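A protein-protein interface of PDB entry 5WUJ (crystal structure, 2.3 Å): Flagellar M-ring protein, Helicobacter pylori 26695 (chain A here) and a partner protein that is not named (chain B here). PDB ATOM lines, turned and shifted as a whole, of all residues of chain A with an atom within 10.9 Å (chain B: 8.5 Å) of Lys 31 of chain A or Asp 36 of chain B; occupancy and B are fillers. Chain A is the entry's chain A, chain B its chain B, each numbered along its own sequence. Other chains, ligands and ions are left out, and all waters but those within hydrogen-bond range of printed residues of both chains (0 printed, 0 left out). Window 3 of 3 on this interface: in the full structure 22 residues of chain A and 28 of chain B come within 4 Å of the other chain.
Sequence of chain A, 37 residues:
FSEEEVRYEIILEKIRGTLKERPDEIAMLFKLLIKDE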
ATOM      1  N   PRO A  23     -17.370 -30.291  -3.885  1.00  0.00           N
ATOM      2  CA  PRO A  23     -16.752 -29.088  -3.307  1.00  0.00           C
ATOM      3  C   PRO A  23     -15.357 -29.327  -2.762  1.00  0.00           C
ATOM      4  O   PRO A  23     -14.496 -28.444  -2.888  1.00  0.00           O
ATOM      5  CB  PRO A  23     -17.736 -28.694  -2.192  1.00  0.00           C
ATOM      6  CG  PRO A  23     -18.480 -29.966  -1.863  1.00  0.00           C
ATOM      7  CD  PRO A  23     -18.647 -30.607  -3.222  1.00  0.00           C
ATOM      8  N   ASP A  24     -15.102 -30.492  -2.157  1.00  0.00           N
ATOM      9  CA  ASP A  24     -13.778 -30.716  -1.590  1.00  0.00           C
ATOM     10  C   ASP A  24     -12.733 -30.846  -2.691  1.00  0.00           C
ATOM     11  O   ASP A  24     -11.629 -30.307  -2.568  1.00  0.00           O
ATOM     12  CB  ASP A  24     -13.777 -31.941  -0.659  1.00  0.00           C
ATOM     13  CG  ASP A  24     -14.281 -33.221  -1.341  1.00  0.00           C
ATOM     14  OD1 ASP A  24     -15.045 -33.124  -2.343  1.00  0.00           O
ATOM     15  OD2 ASP A  24     -13.919 -34.327  -0.858  1.00  0.00           O
ATOM     16  N   GLU A  25     -13.080 -31.500  -3.802  1.00  0.00           N
ATOM     17  CA  GLU A  25     -12.115 -31.638  -4.894  1.00  0.00           C
ATOM     18  C   GLU A  25     -11.844 -30.300  -5.583  1.00  0.00           C
ATOM     19  O   GLU A  25     -10.687 -29.970  -5.862  1.00  0.00           O
ATOM     20  CB  GLU A  25     -12.598 -32.683  -5.904  1.00  0.00           C
ATOM     21  CG  GLU A  25     -12.853 -34.068  -5.284  1.00  0.00           C
ATOM     22  CD  GLU A  25     -13.281 -35.126  -6.312  1.00  0.00           C
ATOM     23  OE1 GLU A  25     -13.338 -34.807  -7.513  1.00  0.00           O
ATOM     24  OE2 GLU A  25     -13.562 -36.280  -5.915  1.00  0.00           O
ATOM     25  N   ILE A  26     -12.886 -29.512  -5.863  1.00  0.00           N
ATOM     26  CA  ILE A  26     -12.660 -28.206  -6.480  1.00  0.00           C
ATOM     27  C   ILE A  26     -11.857 -27.303  -5.553  1.00  0.00           C
ATOM     28  O   ILE A  26     -10.969 -26.565  -5.998  1.00  0.00           O
ATOM     29  CB  ILE A  26     -13.994 -27.544  -6.881  1.00  0.00           C
ATOM     30  CG1 ILE A  26     -14.750 -28.428  -7.867  1.00  0.00           C
ATOM     31  CG2 ILE A  26     -13.720 -26.202  -7.549  1.00  0.00           C
ATOM     32  CD1 ILE A  26     -13.933 -28.824  -9.083  1.00  0.00           C
ATOM     33  N   ALA A  27     -12.150 -27.345  -4.249  1.00  0.00           N
ATOM     34  CA  ALA A  27     -11.365 -26.573  -3.290  1.00  0.00           C
ATOM     35  C   ALA A  27      -9.886 -26.918  -3.385  1.00  0.00           C
ATOM     36  O   ALA A  27      -9.025 -26.032  -3.331  1.00  0.00           O
ATOM     37  CB  ALA A  27     -11.867 -26.818  -1.873  1.00  0.00           C
ATOM     38  N   MET A  28      -9.567 -28.199  -3.540  1.00  0.00           N
ATOM     39  CA  MET A  28      -8.161 -28.552  -3.643  1.00  0.00           C
ATOM     40  C   MET A  28      -7.623 -28.182  -5.017  1.00  0.00           C
ATOM     41  O   MET A  28      -6.473 -27.748  -5.144  1.00  0.00           O
ATOM     42  CB  MET A  28      -7.964 -30.045  -3.367  1.00  0.00           C
ATOM     43  CG  MET A  28      -6.556 -30.561  -3.638  1.00  0.00           C
ATOM     44  SD  MET A  28      -5.308 -29.867  -2.498  1.00  0.00           S
ATOM     45  CE  MET A  28      -6.008 -30.344  -0.942  1.00  0.00           C
ATOM     46  N   LEU A  29      -8.436 -28.353  -6.062  1.00  0.00           N
ATOM     47  CA  LEU A  29      -8.028 -27.868  -7.371  1.00  0.00           C
ATOM     48  C   LEU A  29      -7.631 -26.402  -7.289  1.00  0.00           C
ATOM     49  O   LEU A  29      -6.611 -25.994  -7.853  1.00  0.00           O
ATOM     50  CB  LEU A  29      -9.156 -28.064  -8.388  1.00  0.00           C
ATOM     51  CG  LEU A  29      -8.902 -27.463  -9.769  1.00  0.00           C
ATOM     52  CD1 LEU A  29      -7.861 -28.278 -10.496  1.00  0.00           C
ATOM     53  CD2 LEU A  29     -10.197 -27.439 -10.558  1.00  0.00           C
ATOM     54  N   PHE A  30      -8.414 -25.598  -6.557  1.00  0.00           N
ATOM     55  CA  PHE A  30      -8.098 -24.178  -6.441  1.00  0.00           C
ATOM     56  C   PHE A  30      -6.775 -23.978  -5.716  1.00  0.00           C
ATOM     57  O   PHE A  30      -5.934 -23.179  -6.148  1.00  0.00           O
ATOM     58  CB  PHE A  30      -9.225 -23.435  -5.719  1.00  0.00           C
ATOM     59  CG  PHE A  30     -10.462 -23.258  -6.537  1.00  0.00           C
ATOM     60  CD1 PHE A  30     -10.415 -23.306  -7.919  1.00  0.00           C
ATOM     61  CD2 PHE A  30     -11.691 -23.048  -5.917  1.00  0.00           C
ATOM     62  CE1 PHE A  30     -11.580 -23.127  -8.683  1.00  0.00           C
ATOM     63  CE2 PHE A  30     -12.845 -22.864  -6.659  1.00  0.00           C
ATOM     64  CZ  PHE A  30     -12.791 -22.906  -8.053  1.00  0.00           C
ATOM     65  N   LYS A  31      -6.571 -24.701  -4.607  1.00  0.00           N
ATOM     66  CA  LYS A  31      -5.287 -24.631  -3.915  1.00  0.00           C
ATOM     67  C   LYS A  31      -4.151 -24.994  -4.858  1.00  0.00           C
ATOM     68  O   LYS A  31      -3.141 -24.283  -4.935  1.00  0.00           O
ATOM     69  CB  LYS A  31      -5.277 -25.558  -2.695  1.00  0.00           C
ATOM     70  CG  LYS A  31      -6.079 -25.052  -1.506  1.00  0.00           C
ATOM     71  CD  LYS A  31      -5.887 -25.955  -0.298  1.00  0.00           C
ATOM     72  CE  LYS A  31      -4.426 -26.020   0.080  1.00  0.00           C
ATOM     73  NZ  LYS A  31      -4.209 -26.490   1.472  1.00  0.00           N
ATOM     74  N   LEU A  32      -4.316 -26.086  -5.615  1.00  0.00           N
ATOM     75  CA  LEU A  32      -3.238 -26.525  -6.501  1.00  0.00           C
ATOM     76  C   LEU A  32      -2.989 -25.511  -7.610  1.00  0.00           C
ATOM     77  O   LEU A  32      -1.834 -25.253  -7.973  1.00  0.00           O
ATOM     78  CB  LEU A  32      -3.552 -27.900  -7.092  1.00  0.00           C
ATOM     79  CG  LEU A  32      -3.520 -29.077  -6.118  1.00  0.00           C
ATOM     80  CD1 LEU A  32      -4.164 -30.312  -6.756  1.00  0.00           C
ATOM     81  CD2 LEU A  32      -2.064 -29.353  -5.629  1.00  0.00           C
ATOM     82  N   LEU A  33      -4.058 -24.907  -8.153  1.00  0.00           N
ATOM     83  CA  LEU A  33      -3.868 -23.895  -9.189  1.00  0.00           C
ATOM     84  C   LEU A  33      -3.082 -22.708  -8.646  1.00  0.00           C
ATOM     85  O   LEU A  33      -2.159 -22.208  -9.302  1.00  0.00           O
ATOM     86  CB  LEU A  33      -5.221 -23.445  -9.752  1.00  0.00           C
ATOM     87  CG  LEU A  33      -5.930 -24.450 -10.667  1.00  0.00           C
ATOM     88  CD1 LEU A  33      -7.369 -24.020 -10.962  1.00  0.00           C
ATOM     89  CD2 LEU A  33      -5.155 -24.642 -11.960  1.00  0.00           C
ATOM     90  N   ILE A  34      -3.425 -22.258  -7.435  1.00  0.00           N
ATOM     91  CA  ILE A  34      -2.719 -21.139  -6.819  1.00  0.00           C
ATOM     92  C   ILE A  34      -1.249 -21.485  -6.622  1.00  0.00           C
ATOM     93  O   ILE A  34      -0.357 -20.712  -6.994  1.00  0.00           O
ATOM     94  CB  ILE A  34      -3.380 -20.754  -5.484  1.00  0.00           C
ATOM     95  CG1 ILE A  34      -4.762 -20.129  -5.720  1.00  0.00           C
ATOM     96  CG2 ILE A  34      -2.432 -19.837  -4.671  1.00  0.00           C
ATOM     97  CD1 ILE A  34      -5.533 -19.878  -4.436  1.00  0.00           C
ATOM     98  N   LYS A  35      -0.978 -22.656  -6.029  1.00  0.00           N
ATOM     99  CA  LYS A  35       0.397 -23.065  -5.753  1.00  0.00           C
ATOM    100  C   LYS A  35       1.198 -23.220  -7.039  1.00  0.00           C
ATOM    101  O   LYS A  35       2.408 -22.965  -7.051  1.00  0.00           O
ATOM    102  CB  LYS A  35       0.413 -24.378  -4.963  1.00  0.00           C
ATOM    103  CG  LYS A  35       0.394 -24.211  -3.448  1.00  0.00           C
ATOM    104  CD  LYS A  35      -0.084 -25.483  -2.747  1.00  0.00           C
ATOM    105  CE  LYS A  35       0.000 -25.332  -1.239  1.00  0.00           C
ATOM    106  NZ  LYS A  35       1.388 -24.992  -0.813  1.00  0.00           N
ATOM    107  N   ASP A  36       0.536 -23.631  -8.126  1.00  0.00           N
ATOM    108  CA  ASP A  36       1.192 -23.756  -9.426  1.00  0.00           C
ATOM    109  C   ASP A  36       1.786 -22.426  -9.878  1.00  0.00           C
ATOM    110  O   ASP A  36       2.849 -22.390 -10.510  1.00  0.00           O
ATOM    111  CB  ASP A  36       0.180 -24.277 -10.452  1.00  0.00           C
ATOM    112  CG  ASP A  36       0.771 -24.465 -11.840  1.00  0.00           C
ATOM    113  OD1 ASP A  36       0.891 -25.630 -12.276  1.00  0.00           O
ATOM    114  OD2 ASP A  36       1.087 -23.456 -12.511  1.00  0.00           O
ATOM    115  N   GLU A  37       1.115 -21.327  -9.561  1.00  0.00           N
ATOM    116  CA  GLU A  37       1.503 -20.022 -10.058  1.00  0.00           C
ATOM    117  C   GLU A  37       2.200 -19.202  -8.976  1.00  0.00           C
ATOM    118  O   GLU A  37       3.413 -19.283  -8.815  1.00  0.00           O
ATOM    119  CB  GLU A  37       0.269 -19.290 -10.589  1.00  0.00           C
ATOM    120  CG  GLU A  37       0.279 -17.802 -10.351  1.00  0.00           C
ATOM    121  CD  GLU A  37      -0.940 -17.122 -10.933  1.00  0.00           C
ATOM    122  OE1 GLU A  37      -1.361 -17.500 -12.045  1.00  0.00           O
ATOM    123  OE2 GLU A  37      -1.477 -16.212 -10.274  1.00  0.00           O
ATOM    124  N   MET B  12      -4.053 -15.974 -10.145  1.00  0.00           N
ATOM    125  CA  MET B  12      -4.957 -17.116 -10.152  1.00  0.00           C
ATOM    126  C   MET B  12      -5.936 -17.038  -8.978  1.00  0.00           C
ATOM    127  O   MET B  12      -7.113 -17.399  -9.104  1.00  0.00           O
ATOM    128  CB  MET B  12      -4.136 -18.408 -10.134  1.00  0.00           C
ATOM    129  CG  MET B  12      -4.962 -19.675 -10.099  1.00  0.00           C
ATOM    130  SD  MET B  12      -6.175 -19.758 -11.448  1.00  0.00           S
ATOM    131  CE  MET B  12      -5.154 -20.249 -12.827  1.00  0.00           C
ATOM    132  N   ILE B  16      -9.980 -16.889  -9.098  1.00  0.00           N
ATOM    133  CA  ILE B  16     -10.828 -17.811  -8.346  1.00  0.00           C
ATOM    134  C   ILE B  16     -11.892 -17.047  -7.571  1.00  0.00           C
ATOM    135  O   ILE B  16     -13.056 -17.451  -7.540  1.00  0.00           O
ATOM    136  CB  ILE B  16      -9.963 -18.692  -7.428  1.00  0.00           C
ATOM    137  CG1 ILE B  16      -9.236 -19.761  -8.246  1.00  0.00           C
ATOM    138  CG2 ILE B  16     -10.803 -19.310  -6.320  1.00  0.00           C
ATOM    139  CD1 ILE B  16      -8.002 -20.354  -7.518  1.00  0.00           C
ATOM    140  N   ILE B  31     -17.435 -24.169  -1.054  1.00  0.00           N
ATOM    141  CA  ILE B  31     -16.007 -24.305  -1.337  1.00  0.00           C
ATOM    142  C   ILE B  31     -15.189 -23.892  -0.121  1.00  0.00           C
ATOM    143  O   ILE B  31     -14.270 -24.609   0.304  1.00  0.00           O
ATOM    144  CB  ILE B  31     -15.604 -23.468  -2.563  1.00  0.00           C
ATOM    145  CG1 ILE B  31     -16.222 -24.007  -3.861  1.00  0.00           C
ATOM    146  CG2 ILE B  31     -14.092 -23.483  -2.707  1.00  0.00           C
ATOM    147  CD1 ILE B  31     -16.144 -25.495  -4.016  1.00  0.00           C
ATOM    148  N   LEU B  32     -15.519 -22.727   0.457  1.00  0.00           N
ATOM    149  CA  LEU B  32     -14.728 -22.189   1.563  1.00  0.00           C
ATOM    150  C   LEU B  32     -14.677 -23.151   2.742  1.00  0.00           C
ATOM    151  O   LEU B  32     -13.644 -23.245   3.417  1.00  0.00           O
ATOM    152  CB  LEU B  32     -15.284 -20.846   2.028  1.00  0.00           C
ATOM    153  CG  LEU B  32     -15.345 -19.675   1.051  1.00  0.00           C
ATOM    154  CD1 LEU B  32     -15.844 -18.426   1.774  1.00  0.00           C
ATOM    155  CD2 LEU B  32     -14.006 -19.394   0.384  1.00  0.00           C
ATOM    156  N   ARG B  33     -15.762 -23.893   2.991  1.00  0.00           N
ATOM    157  CA  ARG B  33     -15.792 -24.830   4.110  1.00  0.00           C
ATOM    158  C   ARG B  33     -14.831 -26.003   3.931  1.00  0.00           C
ATOM    159  O   ARG B  33     -14.609 -26.743   4.893  1.00  0.00           O
ATOM    160  CB  ARG B  33     -17.230 -25.342   4.334  1.00  0.00           C
ATOM    161  CG  ARG B  33     -18.192 -24.274   4.902  1.00  0.00           C
ATOM    162  CD  ARG B  33     -19.524 -24.841   5.419  1.00  0.00           C
ATOM    163  NE  ARG B  33     -20.419 -25.255   4.340  1.00  0.00           N
ATOM    164  CZ  ARG B  33     -21.275 -24.450   3.708  1.00  0.00           C
ATOM    165  NH1 ARG B  33     -21.361 -23.162   4.033  1.00  0.00           N
ATOM    166  NH2 ARG B  33     -22.042 -24.932   2.736  1.00  0.00           N
ATOM    167  N   HIS B  34     -14.262 -26.197   2.740  1.00  0.00           N
ATOM    168  CA  HIS B  34     -13.277 -27.243   2.506  1.00  0.00           C
ATOM    169  C   HIS B  34     -11.864 -26.701   2.327  1.00  0.00           C
ATOM    170  O   HIS B  34     -10.946 -27.488   2.067  1.00  0.00           O
ATOM    171  CB  HIS B  34     -13.672 -28.082   1.282  1.00  0.00           C
ATOM    172  CG  HIS B  34     -14.873 -28.943   1.512  1.00  0.00           C
ATOM    173  ND1 HIS B  34     -16.154 -28.534   1.205  1.00  0.00           N
ATOM    174  CD2 HIS B  34     -14.995 -30.182   2.043  1.00  0.00           C
ATOM    175  CE1 HIS B  34     -17.009 -29.485   1.529  1.00  0.00           C
ATOM    176  NE2 HIS B  34     -16.332 -30.500   2.036  1.00  0.00           N
ATOM    177  N   LEU B  35     -11.663 -25.393   2.459  1.00  0.00           N
ATOM    178  CA  LEU B  35     -10.338 -24.800   2.369  1.00  0.00           C
ATOM    179  C   LEU B  35      -9.743 -24.603   3.759  1.00  0.00           C
ATOM    180  O   LEU B  35     -10.453 -24.551   4.766  1.00  0.00           O
ATOM    181  CB  LEU B  35     -10.382 -23.461   1.629  1.00  0.00           C
ATOM    182  CG  LEU B  35     -10.623 -23.568   0.120  1.00  0.00           C
ATOM    183  CD1 LEU B  35     -10.816 -22.184  -0.484  1.00  0.00           C
ATOM    184  CD2 LEU B  35      -9.482 -24.318  -0.567  1.00  0.00           C
ATOM    185  N   ASP B  36      -8.417 -24.487   3.794  1.00  0.00           N
ATOM    186  CA  ASP B  36      -7.671 -24.137   4.995  1.00  0.00           C
ATOM    187  C   ASP B  36      -7.833 -22.643   5.277  1.00  0.00           C
ATOM    188  O   ASP B  36      -8.239 -21.867   4.405  1.00  0.00           O
ATOM    189  CB  ASP B  36      -6.194 -24.486   4.814  1.00  0.00           C
ATOM    190  CG  ASP B  36      -5.565 -23.697   3.668  1.00  0.00           C
ATOM    191  OD1 ASP B  36      -4.877 -22.690   3.931  1.00  0.00           O
ATOM    192  OD2 ASP B  36      -5.810 -24.054   2.492  1.00  0.00           O
ATOM    193  N   ILE B  37      -7.485 -22.232   6.504  1.00  0.00           N
ATOM    194  CA  ILE B  37      -7.748 -20.855   6.933  1.00  0.00           C
ATOM    195  C   ILE B  37      -6.958 -19.860   6.094  1.00  0.00           C
ATOM    196  O   ILE B  37      -7.478 -18.810   5.695  1.00  0.00           O
ATOM    197  CB  ILE B  37      -7.443 -20.680   8.431  1.00  0.00           C
ATOM    198  CG1 ILE B  37      -8.487 -21.405   9.275  1.00  0.00           C
ATOM    199  CG2 ILE B  37      -7.401 -19.195   8.795  1.00  0.00           C
ATOM    200  CD1 ILE B  37      -7.930 -21.965  10.562  1.00  0.00           C
ATOM    201  N   ASP B  38      -5.692 -20.163   5.811  1.00  0.00           N
ATOM    202  CA  ASP B  38      -4.897 -19.234   5.011  1.00  0.00           C
ATOM    203  C   ASP B  38      -5.470 -19.088   3.600  1.00  0.00           C
ATOM    204  O   ASP B  38      -5.526 -17.976   3.058  1.00  0.00           O
ATOM    205  CB  ASP B  38      -3.438 -19.684   4.972  1.00  0.00           C
ATOM    206  CG  ASP B  38      -2.714 -19.408   6.276  1.00  0.00           C
ATOM    207  OD1 ASP B  38      -2.849 -18.283   6.796  1.00  0.00           O
ATOM    208  OD2 ASP B  38      -2.010 -20.312   6.780  1.00  0.00           O
ATOM    209  N   SER B  39      -5.912 -20.194   2.992  1.00  0.00           N
ATOM    210  CA  SER B  39      -6.576 -20.088   1.694  1.00  0.00           C
ATOM    211  C   SER B  39      -7.852 -19.262   1.804  1.00  0.00           C
ATOM    212  O   SER B  39      -8.108 -18.388   0.967  1.00  0.00           O
ATOM    213  CB  SER B  39      -6.875 -21.481   1.121  1.00  0.00           C
ATOM    214  OG  SER B  39      -5.697 -22.098   0.605  1.00  0.00           O
ATOM    215  N   ILE B  40      -8.667 -19.518   2.835  1.00  0.00           N
ATOM    216  CA  ILE B  40      -9.920 -18.773   2.980  1.00  0.00           C
ATOM    217  C   ILE B  40      -9.636 -17.291   3.153  1.00  0.00           C
ATOM    218  O   ILE B  40     -10.348 -16.440   2.606  1.00  0.00           O
ATOM    219  CB  ILE B  40     -10.754 -19.305   4.156  1.00  0.00           C
ATOM    220  CG1 ILE B  40     -11.241 -20.733   3.893  1.00  0.00           C
ATOM    221  CG2 ILE B  40     -11.930 -18.363   4.432  1.00  0.00           C
ATOM    222  CD1 ILE B  40     -11.785 -21.402   5.160  1.00  0.00           C
ATOM    223  N   THR B  41      -8.589 -16.960   3.905  1.00  0.00           N
ATOM    224  CA  THR B  41      -8.244 -15.559   4.122  1.00  0.00           C
ATOM    225  C   THR B  41      -7.933 -14.856   2.809  1.00  0.00           C
ATOM    226  O   THR B  41      -8.435 -13.757   2.547  1.00  0.00           O
ATOM    227  CB  THR B  41      -7.048 -15.451   5.069  1.00  0.00           C
ATOM    228  OG1 THR B  41      -7.354 -16.141   6.287  1.00  0.00           O
ATOM    229  CG2 THR B  41      -6.754 -13.995   5.364  1.00  0.00           C
ATOM    230  N   GLU B  42      -7.081 -15.468   1.980  1.00  0.00           N
ATOM    231  CA  GLU B  42      -6.702 -14.850   0.714  1.00  0.00           C
ATOM    232  C   GLU B  42      -7.900 -14.725  -0.222  1.00  0.00           C
ATOM    233  O   GLU B  42      -8.105 -13.675  -0.840  1.00  0.00           O
ATOM    234  CB  GLU B  42      -5.579 -15.653   0.052  1.00  0.00           C
ATOM    235  CG  GLU B  42      -5.042 -15.030  -1.234  1.00  0.00           C
ATOM    236  CD  GLU B  42      -4.306 -13.723  -0.990  1.00  0.00           C
ATOM    237  OE1 GLU B  42      -4.251 -12.894  -1.923  1.00  0.00           O
ATOM    238  OE2 GLU B  42      -3.784 -13.524   0.132  1.00  0.00           O
ATOM    239  N   ILE B  43      -8.724 -15.770  -0.314  1.00  0.00           N
ATOM    240  CA  ILE B  43      -9.825 -15.742  -1.271  1.00  0.00           C
ATOM    241  C   ILE B  43     -10.915 -14.782  -0.806  1.00  0.00           C
ATOM    242  O   ILE B  43     -11.434 -13.982  -1.596  1.00  0.00           O
ATOM    243  CB  ILE B  43     -10.349 -17.173  -1.499  1.00  0.00           C
ATOM    244  CG1 ILE B  43      -9.354 -17.939  -2.366  1.00  0.00           C
ATOM    245  CG2 ILE B  43     -11.714 -17.150  -2.177  1.00  0.00           C
ATOM    246  CD1 ILE B  43      -9.802 -19.340  -2.732  1.00  0.00           C
ATOM    247  N   SER B  44     -11.255 -14.826   0.489  1.00  0.00           N
ATOM    248  CA  SER B  44     -12.210 -13.882   1.069  1.00  0.00           C
ATOM    249  C   SER B  44     -11.785 -12.443   0.824  1.00  0.00           C
ATOM    250  O   SER B  44     -12.623 -11.575   0.538  1.00  0.00           O
ATOM    251  CB  SER B  44     -12.339 -14.122   2.578  1.00  0.00           C
ATOM    252  OG  SER B  44     -12.897 -15.395   2.835  1.00  0.00           O
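NZ of Lys 31 of chain A lies within salt-bridge range of OD2 of Asp 36 of chain B (3.1 Å).
The backbone NH of Met 12 of chain B lies within hydrogen-bond range of the side-chain carboxylate of Glu 37 of chain A, 2.6 Å away.
The side-chain carboxylate (OD2) of Asp 36 of chain B lies within hydrogen-bond range of the side-chain hydroxyl (OG) of Ser 39 of chain B (2.7 Å).
The side-chain carboxylate (OD1) of Asp 36 of chain B lies within hydrogen-bond range of the backbone NH (N) of Asp 38 of chain B, 3.3 Å away.
O of Pro 23 of chain A touches CD1 of Ile 31 of chain B, 3.6 Å away.
CE1 of His 34 of chain B touches CG of Pro 23 of chain A (3.7 Å).
His 34 of chain B touches Asp 24 of chain A.
CB of Ala 27 of chain A touches O of Ile 31 of chain B (3.9 Å).
Ala 27 of chain A touches His 34 of chain B.
Ala 27 of chain A touches Leu 35 of chain B (O to CD2, 3.3 Å).
CG of Lys 31 of chain A touches CD2 of Leu 35 of chain B (3.6 Å).
Ser 39 of chain B touches Lys 31 of chain A.
CB of Leu 33 of chain A touches CG of Met 12 of chain B (3.8 Å).
CG1 of Ile 34 of chain A touches CD1 of Ile 16 of chain B (3.7 Å).
Of chain A, only Lys 31 (3.1 Å) comes within 4 Å of Asp 36 of chain B.
Leu 35 of chain B touches just these residues of chain A: Ala 27 (3.3 Å) and Lys 31 (3.6 Å).
No residue of chain A comes within 4 Å of Ile 37 of chain B.
Asp 38 of chain B touches none of the printed residues of chain A.
Of chain A, only Lys 31 (3.7 Å) comes within 4 Å of Ser 39 of chain B.
Ile 40 of chain B touches none of the printed residues of chain A.
Printed residues of chain B within 4 Å of Ala 27 of chain A: Ile 31, His 34 and Leu 35.
Printed residues of chain A within 4 Å of Met 12 of chain B: Leu 33 (3.8 Å) and Glu 37 (2.6 Å).
Printed residues of chain B within 4 Å of Ile 34 of chain A: Ile 16 (3.7 Å).
Of the printed residues of chain A, Ile 16 of chain B touches Phe 30 and Ile 34.
Leu 32 of chain B touches none of the printed residues of chain A.
Met 28 of chain A touches none of the printed residues of chain B.
The nearest residue of chain A that does not touch Asp 36 of chain B is Ala 27 of chain A (6.9 Å).
The nearest printed residue of chain B that does not touch Ile 34 of chain A is Met 12 of chain B (4.02 Å).
Of the 15 printed residues of chain A, 8 touch a printed residue of chain B.
Of the 16 printed residues of chain B, 7 touch a printed residue of chain A.
Hydrophobic or aromatic side chains of chain B that line the printed part of chain A: Met 12, Ile 16, Ile 31, His 34 and Leu 35.
Among the printed residues, Asp or Glu carboxylates within 4 Å of a Lys or Arg side-chain nitrogen of the other chain: Lys 31 of chain A with Asp 36 of chain B.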
